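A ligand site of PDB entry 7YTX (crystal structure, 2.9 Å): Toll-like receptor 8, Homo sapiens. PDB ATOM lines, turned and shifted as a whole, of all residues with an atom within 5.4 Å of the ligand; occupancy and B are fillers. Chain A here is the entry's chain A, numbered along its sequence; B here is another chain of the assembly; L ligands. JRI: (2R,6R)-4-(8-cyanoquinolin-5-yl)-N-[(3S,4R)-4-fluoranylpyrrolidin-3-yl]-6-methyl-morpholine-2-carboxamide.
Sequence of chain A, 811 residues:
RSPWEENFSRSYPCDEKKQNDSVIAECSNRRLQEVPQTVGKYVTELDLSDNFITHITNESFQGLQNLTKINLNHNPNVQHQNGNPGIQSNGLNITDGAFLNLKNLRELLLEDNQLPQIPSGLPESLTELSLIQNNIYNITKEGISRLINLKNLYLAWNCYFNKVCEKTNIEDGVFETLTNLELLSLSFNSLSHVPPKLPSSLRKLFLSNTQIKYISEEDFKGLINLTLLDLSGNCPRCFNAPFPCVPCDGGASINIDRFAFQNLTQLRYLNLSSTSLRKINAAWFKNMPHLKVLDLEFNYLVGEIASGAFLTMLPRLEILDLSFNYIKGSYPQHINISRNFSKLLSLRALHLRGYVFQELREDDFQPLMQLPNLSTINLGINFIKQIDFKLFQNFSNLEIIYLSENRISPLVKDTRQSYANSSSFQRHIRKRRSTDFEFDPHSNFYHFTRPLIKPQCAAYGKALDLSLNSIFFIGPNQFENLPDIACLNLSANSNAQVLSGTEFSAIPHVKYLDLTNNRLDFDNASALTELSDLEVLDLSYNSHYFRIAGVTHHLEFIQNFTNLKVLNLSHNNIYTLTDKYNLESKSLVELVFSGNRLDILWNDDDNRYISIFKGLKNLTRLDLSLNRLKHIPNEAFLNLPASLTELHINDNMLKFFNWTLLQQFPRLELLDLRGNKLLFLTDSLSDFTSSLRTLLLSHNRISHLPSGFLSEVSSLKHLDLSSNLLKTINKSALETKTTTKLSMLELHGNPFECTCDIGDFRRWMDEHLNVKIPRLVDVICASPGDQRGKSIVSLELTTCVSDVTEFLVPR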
ATOM      1  N   PHE A 239       8.592   3.766  36.836  1.00  0.00           N
ATOM      2  CA  PHE A 239       8.339   3.446  35.433  1.00  0.00           C
ATOM      3  C   PHE A 239       9.486   2.626  34.850  1.00  0.00           C
ATOM      4  O   PHE A 239      10.540   3.167  34.506  1.00  0.00           O
ATOM      5  CB  PHE A 239       8.045   4.679  34.578  1.00  0.00           C
ATOM      6  CG  PHE A 239       7.477   4.357  33.210  1.00  0.00           C
ATOM      7  CD1 PHE A 239       6.118   4.109  33.047  1.00  0.00           C
ATOM      8  CD2 PHE A 239       8.297   4.256  32.105  1.00  0.00           C
ATOM      9  CE1 PHE A 239       5.589   3.793  31.803  1.00  0.00           C
ATOM     10  CE2 PHE A 239       7.765   3.950  30.862  1.00  0.00           C
ATOM     11  CZ  PHE A 239       6.415   3.715  30.705  1.00  0.00           C
ATOM     12  N   ASN A 240       9.259   1.307  34.762  1.00  0.00           N
ATOM     13  CA  ASN A 240      10.084   0.399  33.988  1.00  0.00           C
ATOM     14  C   ASN A 240      11.340   0.043  34.756  1.00  0.00           C
ATOM     15  O   ASN A 240      12.247  -0.563  34.194  1.00  0.00           O
ATOM     16  CB  ASN A 240      10.401   0.967  32.605  1.00  0.00           C
ATOM     17  CG  ASN A 240      10.397  -0.077  31.506  1.00  0.00           C
ATOM     18  OD1 ASN A 240       9.562  -0.027  30.611  1.00  0.00           O
ATOM     19  ND2 ASN A 240      11.327  -1.023  31.555  1.00  0.00           N
ATOM     20  N   PHE A 324      10.230  11.356  30.546  1.00  0.00           N
ATOM     21  CA  PHE A 324       9.311  10.603  31.392  1.00  0.00           C
ATOM     22  C   PHE A 324       8.966  11.416  32.633  1.00  0.00           C
ATOM     23  O   PHE A 324       9.276  11.040  33.769  1.00  0.00           O
ATOM     24  CB  PHE A 324       9.819   9.168  31.599  1.00  0.00           C
ATOM     25  CG  PHE A 324      10.076   8.487  30.285  1.00  0.00           C
ATOM     26  CD1 PHE A 324       9.020   8.078  29.479  1.00  0.00           C
ATOM     27  CD2 PHE A 324      11.373   8.368  29.792  1.00  0.00           C
ATOM     28  CE1 PHE A 324       9.260   7.515  28.226  1.00  0.00           C
ATOM     29  CE2 PHE A 324      11.610   7.814  28.540  1.00  0.00           C
ATOM     30  CZ  PHE A 324      10.550   7.381  27.759  1.00  0.00           C
ATOM     31  N   TYR A 326       5.635  12.827  32.284  1.00  0.00           N
ATOM     32  CA  TYR A 326       4.232  12.964  31.934  1.00  0.00           C
ATOM     33  C   TYR A 326       3.349  12.762  33.174  1.00  0.00           C
ATOM     34  O   TYR A 326       3.812  12.294  34.215  1.00  0.00           O
ATOM     35  CB  TYR A 326       3.868  11.968  30.832  1.00  0.00           C
ATOM     36  CG  TYR A 326       3.789  10.534  31.299  1.00  0.00           C
ATOM     37  CD1 TYR A 326       4.934   9.796  31.581  1.00  0.00           C
ATOM     38  CD2 TYR A 326       2.559   9.910  31.481  1.00  0.00           C
ATOM     39  CE1 TYR A 326       4.856   8.480  32.016  1.00  0.00           C
ATOM     40  CE2 TYR A 326       2.469   8.600  31.921  1.00  0.00           C
ATOM     41  CZ  TYR A 326       3.622   7.886  32.187  1.00  0.00           C
ATOM     42  OH  TYR A 326       3.529   6.576  32.617  1.00  0.00           O
ATOM     43  N   ILE A 327       2.048  13.144  33.035  1.00  0.00           N
ATOM     44  CA  ILE A 327       1.033  12.930  34.058  1.00  0.00           C
ATOM     45  C   ILE A 327       0.050  11.840  33.611  1.00  0.00           C
ATOM     46  O   ILE A 327      -0.504  11.889  32.510  1.00  0.00           O
ATOM     47  CB  ILE A 327       0.309  14.250  34.470  1.00  0.00           C
ATOM     48  CG1 ILE A 327       1.244  15.424  34.821  1.00  0.00           C
ATOM     49  CG2 ILE A 327      -0.724  13.984  35.569  1.00  0.00           C
ATOM     50  CD1 ILE A 327       1.773  15.444  36.249  1.00  0.00           C
ATOM     51  N   LYS A 328      -0.202  10.865  34.496  1.00  0.00           N
ATOM     52  CA  LYS A 328      -0.957   9.692  34.085  1.00  0.00           C
ATOM     53  C   LYS A 328      -2.455   9.984  33.997  1.00  0.00           C
ATOM     54  O   LYS A 328      -3.018  10.736  34.801  1.00  0.00           O
ATOM     55  CB  LYS A 328      -0.603   8.498  34.979  1.00  0.00           C
ATOM     56  CG  LYS A 328      -0.318   8.847  36.432  1.00  0.00           C
ATOM     57  CD  LYS A 328      -0.021   7.626  37.274  1.00  0.00           C
ATOM     58  CE  LYS A 328      -1.068   6.531  37.132  1.00  0.00           C
ATOM     59  NZ  LYS A 328      -2.372   6.918  37.703  1.00  0.00           N
ATOM     60  N   GLY A 329      -3.105   9.329  33.021  1.00  0.00           N
ATOM     61  CA  GLY A 329      -4.473   9.608  32.604  1.00  0.00           C
ATOM     62  C   GLY A 329      -4.521  10.642  31.487  1.00  0.00           C
ATOM     63  O   GLY A 329      -5.482  10.687  30.694  1.00  0.00           O
ATOM     64  N   SER A 330      -3.447  11.442  31.384  1.00  0.00           N
ATOM     65  CA  SER A 330      -3.447  12.665  30.599  1.00  0.00           C
ATOM     66  C   SER A 330      -2.774  12.454  29.237  1.00  0.00           C
ATOM     67  O   SER A 330      -1.805  11.719  29.124  1.00  0.00           O
ATOM     68  CB  SER A 330      -2.811  13.791  31.370  1.00  0.00           C
ATOM     69  OG  SER A 330      -2.823  14.987  30.614  1.00  0.00           O
ATOM     70  N   TYR A 331      -3.304  13.131  28.216  1.00  0.00           N
ATOM     71  CA  TYR A 331      -2.775  13.167  26.858  1.00  0.00           C
ATOM     72  C   TYR A 331      -2.992  14.581  26.292  1.00  0.00           C
ATOM     73  O   TYR A 331      -3.816  14.762  25.371  1.00  0.00           O
ATOM     74  CB  TYR A 331      -3.462  12.057  26.061  1.00  0.00           C
ATOM     75  CG  TYR A 331      -2.999  11.768  24.647  1.00  0.00           C
ATOM     76  CD1 TYR A 331      -1.665  11.728  24.284  1.00  0.00           C
ATOM     77  CD2 TYR A 331      -3.946  11.445  23.684  1.00  0.00           C
ATOM     78  CE1 TYR A 331      -1.286  11.416  22.979  1.00  0.00           C
ATOM     79  CE2 TYR A 331      -3.575  11.129  22.383  1.00  0.00           C
ATOM     80  CZ  TYR A 331      -2.244  11.110  22.030  1.00  0.00           C
ATOM     81  OH  TYR A 331      -1.961  10.775  20.721  1.00  0.00           O
ATOM     82  N   GLY A 354       8.451  11.166  26.680  1.00  0.00           N
ATOM     83  CA  GLY A 354       7.361  10.817  27.571  1.00  0.00           C
ATOM     84  C   GLY A 354       6.883  12.010  28.381  1.00  0.00           C
ATOM     85  O   GLY A 354       6.752  11.914  29.601  1.00  0.00           O
ATOM     86  N   VAL A 356       4.229  13.108  26.397  1.00  0.00           N
ATOM     87  CA  VAL A 356       3.002  12.567  25.808  1.00  0.00           C
ATOM     88  C   VAL A 356       2.023  13.697  25.549  1.00  0.00           C
ATOM     89  O   VAL A 356       1.472  14.288  26.489  1.00  0.00           O
ATOM     90  CB  VAL A 356       2.342  11.436  26.648  1.00  0.00           C
ATOM     91  CG1 VAL A 356       1.113  10.823  25.990  1.00  0.00           C
ATOM     92  CG2 VAL A 356       3.353  10.362  27.030  1.00  0.00           C
ATOM     93  N   ILE A 381       8.871   8.715  22.206  1.00  0.00           N
ATOM     94  CA  ILE A 381       7.783   8.171  23.015  1.00  0.00           C
ATOM     95  C   ILE A 381       6.897   9.315  23.514  1.00  0.00           C
ATOM     96  O   ILE A 381       6.621   9.446  24.719  1.00  0.00           O
ATOM     97  CB  ILE A 381       8.319   7.268  24.158  1.00  0.00           C
ATOM     98  CG1 ILE A 381       9.282   6.169  23.690  1.00  0.00           C
ATOM     99  CG2 ILE A 381       7.159   6.699  24.965  1.00  0.00           C
ATOM    100  CD1 ILE A 381      10.736   6.499  23.907  1.00  0.00           C
ATOM    101  N   PHE A 383       4.161   9.868  21.552  1.00  0.00           N
ATOM    102  CA  PHE A 383       2.922   9.507  20.866  1.00  0.00           C
ATOM    103  C   PHE A 383       2.310  10.758  20.252  1.00  0.00           C
ATOM    104  O   PHE A 383       1.168  11.087  20.560  1.00  0.00           O
ATOM    105  CB  PHE A 383       1.914   8.813  21.796  1.00  0.00           C
ATOM    106  CG  PHE A 383       2.441   7.592  22.506  1.00  0.00           C
ATOM    107  CD1 PHE A 383       2.515   6.362  21.844  1.00  0.00           C
ATOM    108  CD2 PHE A 383       2.924   7.678  23.796  1.00  0.00           C
ATOM    109  CE1 PHE A 383       3.067   5.248  22.460  1.00  0.00           C
ATOM    110  CE2 PHE A 383       3.467   6.572  24.426  1.00  0.00           C
ATOM    111  CZ  PHE A 383       3.531   5.360  23.755  1.00  0.00           C
ATOM    112  N   GLU A 405       8.870   6.628  17.770  1.00  0.00           N
ATOM    113  CA  GLU A 405       7.923   6.193  18.795  1.00  0.00           C
ATOM    114  C   GLU A 405       6.830   7.253  18.973  1.00  0.00           C
ATOM    115  O   GLU A 405       6.312   7.488  20.069  1.00  0.00           O
ATOM    116  CB  GLU A 405       8.633   5.817  20.098  1.00  0.00           C
ATOM    117  CG  GLU A 405       9.406   4.506  20.032  1.00  0.00           C
ATOM    118  CD  GLU A 405       8.824   3.370  20.864  1.00  0.00           C
ATOM    119  OE1 GLU A 405       7.722   2.860  20.492  1.00  0.00           O
ATOM    120  OE2 GLU A 405       9.454   3.021  21.916  1.00  0.00           O
ATOM    121  N   PHE B 472      -2.948   3.181  23.717  1.00  0.00           N
ATOM    122  CA  PHE B 472      -1.801   2.787  24.519  1.00  0.00           C
ATOM    123  C   PHE B 472      -2.093   2.865  26.024  1.00  0.00           C
ATOM    124  O   PHE B 472      -1.335   2.319  26.827  1.00  0.00           O
ATOM    125  CB  PHE B 472      -0.552   3.576  24.113  1.00  0.00           C
ATOM    126  CG  PHE B 472      -0.671   5.076  24.158  1.00  0.00           C
ATOM    127  CD1 PHE B 472      -1.178   5.774  23.073  1.00  0.00           C
ATOM    128  CD2 PHE B 472      -0.289   5.780  25.298  1.00  0.00           C
ATOM    129  CE1 PHE B 472      -1.279   7.164  23.120  1.00  0.00           C
ATOM    130  CE2 PHE B 472      -0.388   7.160  25.345  1.00  0.00           C
ATOM    131  CZ  PHE B 472      -0.886   7.851  24.247  1.00  0.00           C
ATOM    132  N   PHE B 473      -3.137   3.615  26.379  1.00  0.00           N
ATOM    133  CA  PHE B 473      -3.760   3.602  27.697  1.00  0.00           C
ATOM    134  C   PHE B 473      -5.244   3.887  27.443  1.00  0.00           C
ATOM    135  O   PHE B 473      -5.622   4.124  26.301  1.00  0.00           O
ATOM    136  CB  PHE B 473      -3.110   4.584  28.679  1.00  0.00           C
ATOM    137  CG  PHE B 473      -3.509   6.016  28.430  1.00  0.00           C
ATOM    138  CD1 PHE B 473      -2.927   6.749  27.415  1.00  0.00           C
ATOM    139  CD2 PHE B 473      -4.512   6.611  29.190  1.00  0.00           C
ATOM    140  CE1 PHE B 473      -3.301   8.072  27.186  1.00  0.00           C
ATOM    141  CE2 PHE B 473      -4.908   7.916  28.950  1.00  0.00           C
ATOM    142  CZ  PHE B 473      -4.298   8.648  27.946  1.00  0.00           C
ATOM    143  N   SER B 494      -0.895  -2.306  22.862  1.00  0.00           N
ATOM    144  CA  SER B 494       0.257  -2.057  23.708  1.00  0.00           C
ATOM    145  C   SER B 494      -0.139  -1.183  24.879  1.00  0.00           C
ATOM    146  O   SER B 494       0.579  -0.251  25.215  1.00  0.00           O
ATOM    147  CB  SER B 494       1.372  -1.474  22.940  1.00  0.00           C
ATOM    148  OG  SER B 494       1.990  -2.517  22.213  1.00  0.00           O
ATOM    149  N   ALA B 496      -0.721   0.167  28.319  1.00  0.00           N
ATOM    150  CA  ALA B 496       0.135   0.173  29.504  1.00  0.00           C
ATOM    151  C   ALA B 496      -0.614   0.693  30.731  1.00  0.00           C
ATOM    152  O   ALA B 496      -0.013   0.830  31.799  1.00  0.00           O
ATOM    153  CB  ALA B 496       1.369   0.983  29.220  1.00  0.00           C
ATOM    154  N   GLN B 497      -1.920   0.959  30.560  1.00  0.00           N
ATOM    155  CA  GLN B 497      -2.854   1.395  31.597  1.00  0.00           C
ATOM    156  C   GLN B 497      -2.606   0.702  32.943  1.00  0.00           C
ATOM    157  O   GLN B 497      -2.707  -0.521  33.046  1.00  0.00           O
ATOM    158  CB  GLN B 497      -4.295   1.069  31.170  1.00  0.00           C
ATOM    159  CG  GLN B 497      -5.385   1.747  32.011  1.00  0.00           C
ATOM    160  CD  GLN B 497      -5.273   3.264  31.998  1.00  0.00           C
ATOM    161  OE1 GLN B 497      -5.475   3.924  30.981  1.00  0.00           O
ATOM    162  NE2 GLN B 497      -4.939   3.825  33.147  1.00  0.00           N
ATOM    163  N   VAL B 498      -2.332   1.501  33.988  1.00  0.00           N
ATOM    164  CA  VAL B 498      -2.561   1.006  35.342  1.00  0.00           C
ATOM    165  C   VAL B 498      -4.065   0.901  35.557  1.00  0.00           C
ATOM    166  O   VAL B 498      -4.801   1.869  35.334  1.00  0.00           O
ATOM    167  CB  VAL B 498      -1.890   1.840  36.468  1.00  0.00           C
ATOM    168  CG1 VAL B 498      -1.785   1.029  37.750  1.00  0.00           C
ATOM    169  CG2 VAL B 498      -0.529   2.391  36.101  1.00  0.00           C
ATOM    170  N   TYR B 545       4.512  -1.904  33.253  1.00  0.00           N
ATOM    171  CA  TYR B 545       5.713  -1.116  33.392  1.00  0.00           C
ATOM    172  C   TYR B 545       5.824  -0.527  34.797  1.00  0.00           C
ATOM    173  O   TYR B 545       6.499   0.493  34.993  1.00  0.00           O
ATOM    174  CB  TYR B 545       5.716   0.035  32.386  1.00  0.00           C
ATOM    175  CG  TYR B 545       5.812  -0.365  30.929  1.00  0.00           C
ATOM    176  CD1 TYR B 545       6.960  -0.934  30.400  1.00  0.00           C
ATOM    177  CD2 TYR B 545       4.747  -0.131  30.075  1.00  0.00           C
ATOM    178  CE1 TYR B 545       7.053  -1.257  29.057  1.00  0.00           C
ATOM    179  CE2 TYR B 545       4.815  -0.451  28.730  1.00  0.00           C
ATOM    180  CZ  TYR B 545       5.970  -1.019  28.220  1.00  0.00           C
ATOM    181  OH  TYR B 545       5.985  -1.337  26.885  1.00  0.00           O
ATOM    182  N   PHE B 546       5.162  -1.138  35.779  1.00  0.00           N
ATOM    183  CA  PHE B 546       5.110  -0.515  37.094  1.00  0.00           C
ATOM    184  C   PHE B 546       5.370  -1.539  38.183  1.00  0.00           C
ATOM    185  O   PHE B 546       4.586  -1.671  39.120  1.00  0.00           O
ATOM    186  CB  PHE B 546       3.800   0.258  37.325  1.00  0.00           C
ATOM    187  CG  PHE B 546       3.334   1.111  36.169  1.00  0.00           C
ATOM    188  CD1 PHE B 546       2.692   0.549  35.075  1.00  0.00           C
ATOM    189  CD2 PHE B 546       3.562   2.476  36.166  1.00  0.00           C
ATOM    190  CE1 PHE B 546       2.284   1.333  33.999  1.00  0.00           C
ATOM    191  CE2 PHE B 546       3.154   3.260  35.090  1.00  0.00           C
ATOM    192  CZ  PHE B 546       2.514   2.687  34.017  1.00  0.00           C
HETATM  193  C1  JRI L   1       8.940   1.277  25.791  1.00  0.00           C
HETATM  194  C10 JRI L   1       5.766   7.641  28.161  1.00  0.00           C
HETATM  195  C11 JRI L   1       1.496   5.588  29.676  1.00  0.00           C
HETATM  196  C12 JRI L   1       1.151   4.422  30.365  1.00  0.00           C
HETATM  197  C13 JRI L   1       0.018   4.360  31.153  1.00  0.00           C
HETATM  198  C14 JRI L   1      -0.827   5.442  31.286  1.00  0.00           C
HETATM  199  C15 JRI L   1      -0.518   6.658  30.608  1.00  0.00           C
HETATM  200  C16 JRI L   1       0.646   6.732  29.796  1.00  0.00           C
HETATM  201  C17 JRI L   1       0.920   7.936  29.132  1.00  0.00           C
HETATM  202  C18 JRI L   1      -1.050   8.817  30.116  1.00  0.00           C
HETATM  203  C19 JRI L   1       0.075   8.985  29.290  1.00  0.00           C
HETATM  204  C2  JRI L   1       7.071   2.467  24.926  1.00  0.00           C
HETATM  205  C20 JRI L   1      -1.996   5.323  32.103  1.00  0.00           C
HETATM  206  C3  JRI L   1       6.837   2.081  26.391  1.00  0.00           C
HETATM  207  C4  JRI L   1       8.264   1.974  26.933  1.00  0.00           C
HETATM  208  C5  JRI L   1       4.048   4.569  27.145  1.00  0.00           C
HETATM  209  C6  JRI L   1       3.185   4.353  28.367  1.00  0.00           C
HETATM  210  C7  JRI L   1       3.665   6.655  29.063  1.00  0.00           C
HETATM  211  C8  JRI L   1       4.541   6.833  27.839  1.00  0.00           C
HETATM  212  C9  JRI L   1       4.704   3.291  26.691  1.00  0.00           C
HETATM  213  F1  JRI L   1       8.916   3.196  27.165  1.00  0.00           F
HETATM  214  N1  JRI L   1       8.390   1.915  24.577  1.00  0.00           N
HETATM  215  N2  JRI L   1       5.941   2.978  27.119  1.00  0.00           N
HETATM  216  N3  JRI L   1       2.635   5.621  28.877  1.00  0.00           N
HETATM  217  N4  JRI L   1      -1.367   7.716  30.766  1.00  0.00           N
HETATM  218  N5  JRI L   1      -2.952   5.296  32.744  1.00  0.00           N
HETATM  219  O1  JRI L   1       5.050   5.546  27.432  1.00  0.00           O
HETATM  220  O2  JRI L   1       4.077   2.604  25.881  1.00  0.00           O
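The backbone carbonyl oxygen of Gly 354 is in hydrogen-bond range of the backbone NH of Tyr 326, 3.0 Å away.
The backbone NH (N) of Gly 354 lies within hydrogen-bond range of the backbone carbonyl oxygen (O) of Ile 381 (3.2 Å).
The backbone NH of Asn 240 lies within hydrogen-bond range of the backbone carbonyl oxygen of Tyr 545 of chain B, 2.9 Å away.
The backbone carbonyl oxygen of Phe 383 is in hydrogen-bond range of the side-chain hydroxyl of Tyr 331 (3.1 Å).
The backbone NH of Ala 496 of chain B is in hydrogen-bond range of the backbone carbonyl oxygen of Phe 472 of chain B (2.7 Å).
The side-chain carboxylate (OE2) of Glu 405 lies within salt-bridge range of a nitrogen (N1) of the ligand, at 3.1 Å.
N5 of the ligand is in hydrogen-bond range of NE2 of Gln 497 of chain B.
The backbone NH (N) of Gly 329 lies within hydrogen-bond range of a nitrogen (N4) of the ligand (3.3 Å).
Residues that only touch the ligand: Ser 330 (3.2 Å), Tyr 326 (3.3 Å), Phe 383 (3.4 Å), Ile 381 (3.4 Å), Phe 324 (3.5 Å), Tyr 545 of chain B (3.6 Å), Phe 473 of chain B (3.6 Å), Ala 496 of chain B (3.6 Å), Gly 354 (3.6 Å), Phe 239 (3.7 Å), Val 356 (3.8 Å), Lys 328 (3.9 Å) and Ile 327 (3.9 Å).
Hydrophobic or aromatic side chains that line the ligand: Phe 239, Phe 324, Tyr 326, Val 356, Ile 381, Phe 383, Phe 473 of chain B, Ala 496 of chain B and Tyr 545 of chain B.
Within 4 Å of the ligand: Phe 239, Phe 324, Tyr 326, Ile 327, Lys 328, Gly 329, Ser 330, Gly 354, Val 356, Ile 381, Phe 383, Glu 405, Phe 473 of chain B, Ala 496 of chain B, Gln 497 of chain B and Tyr 545 of chain B.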
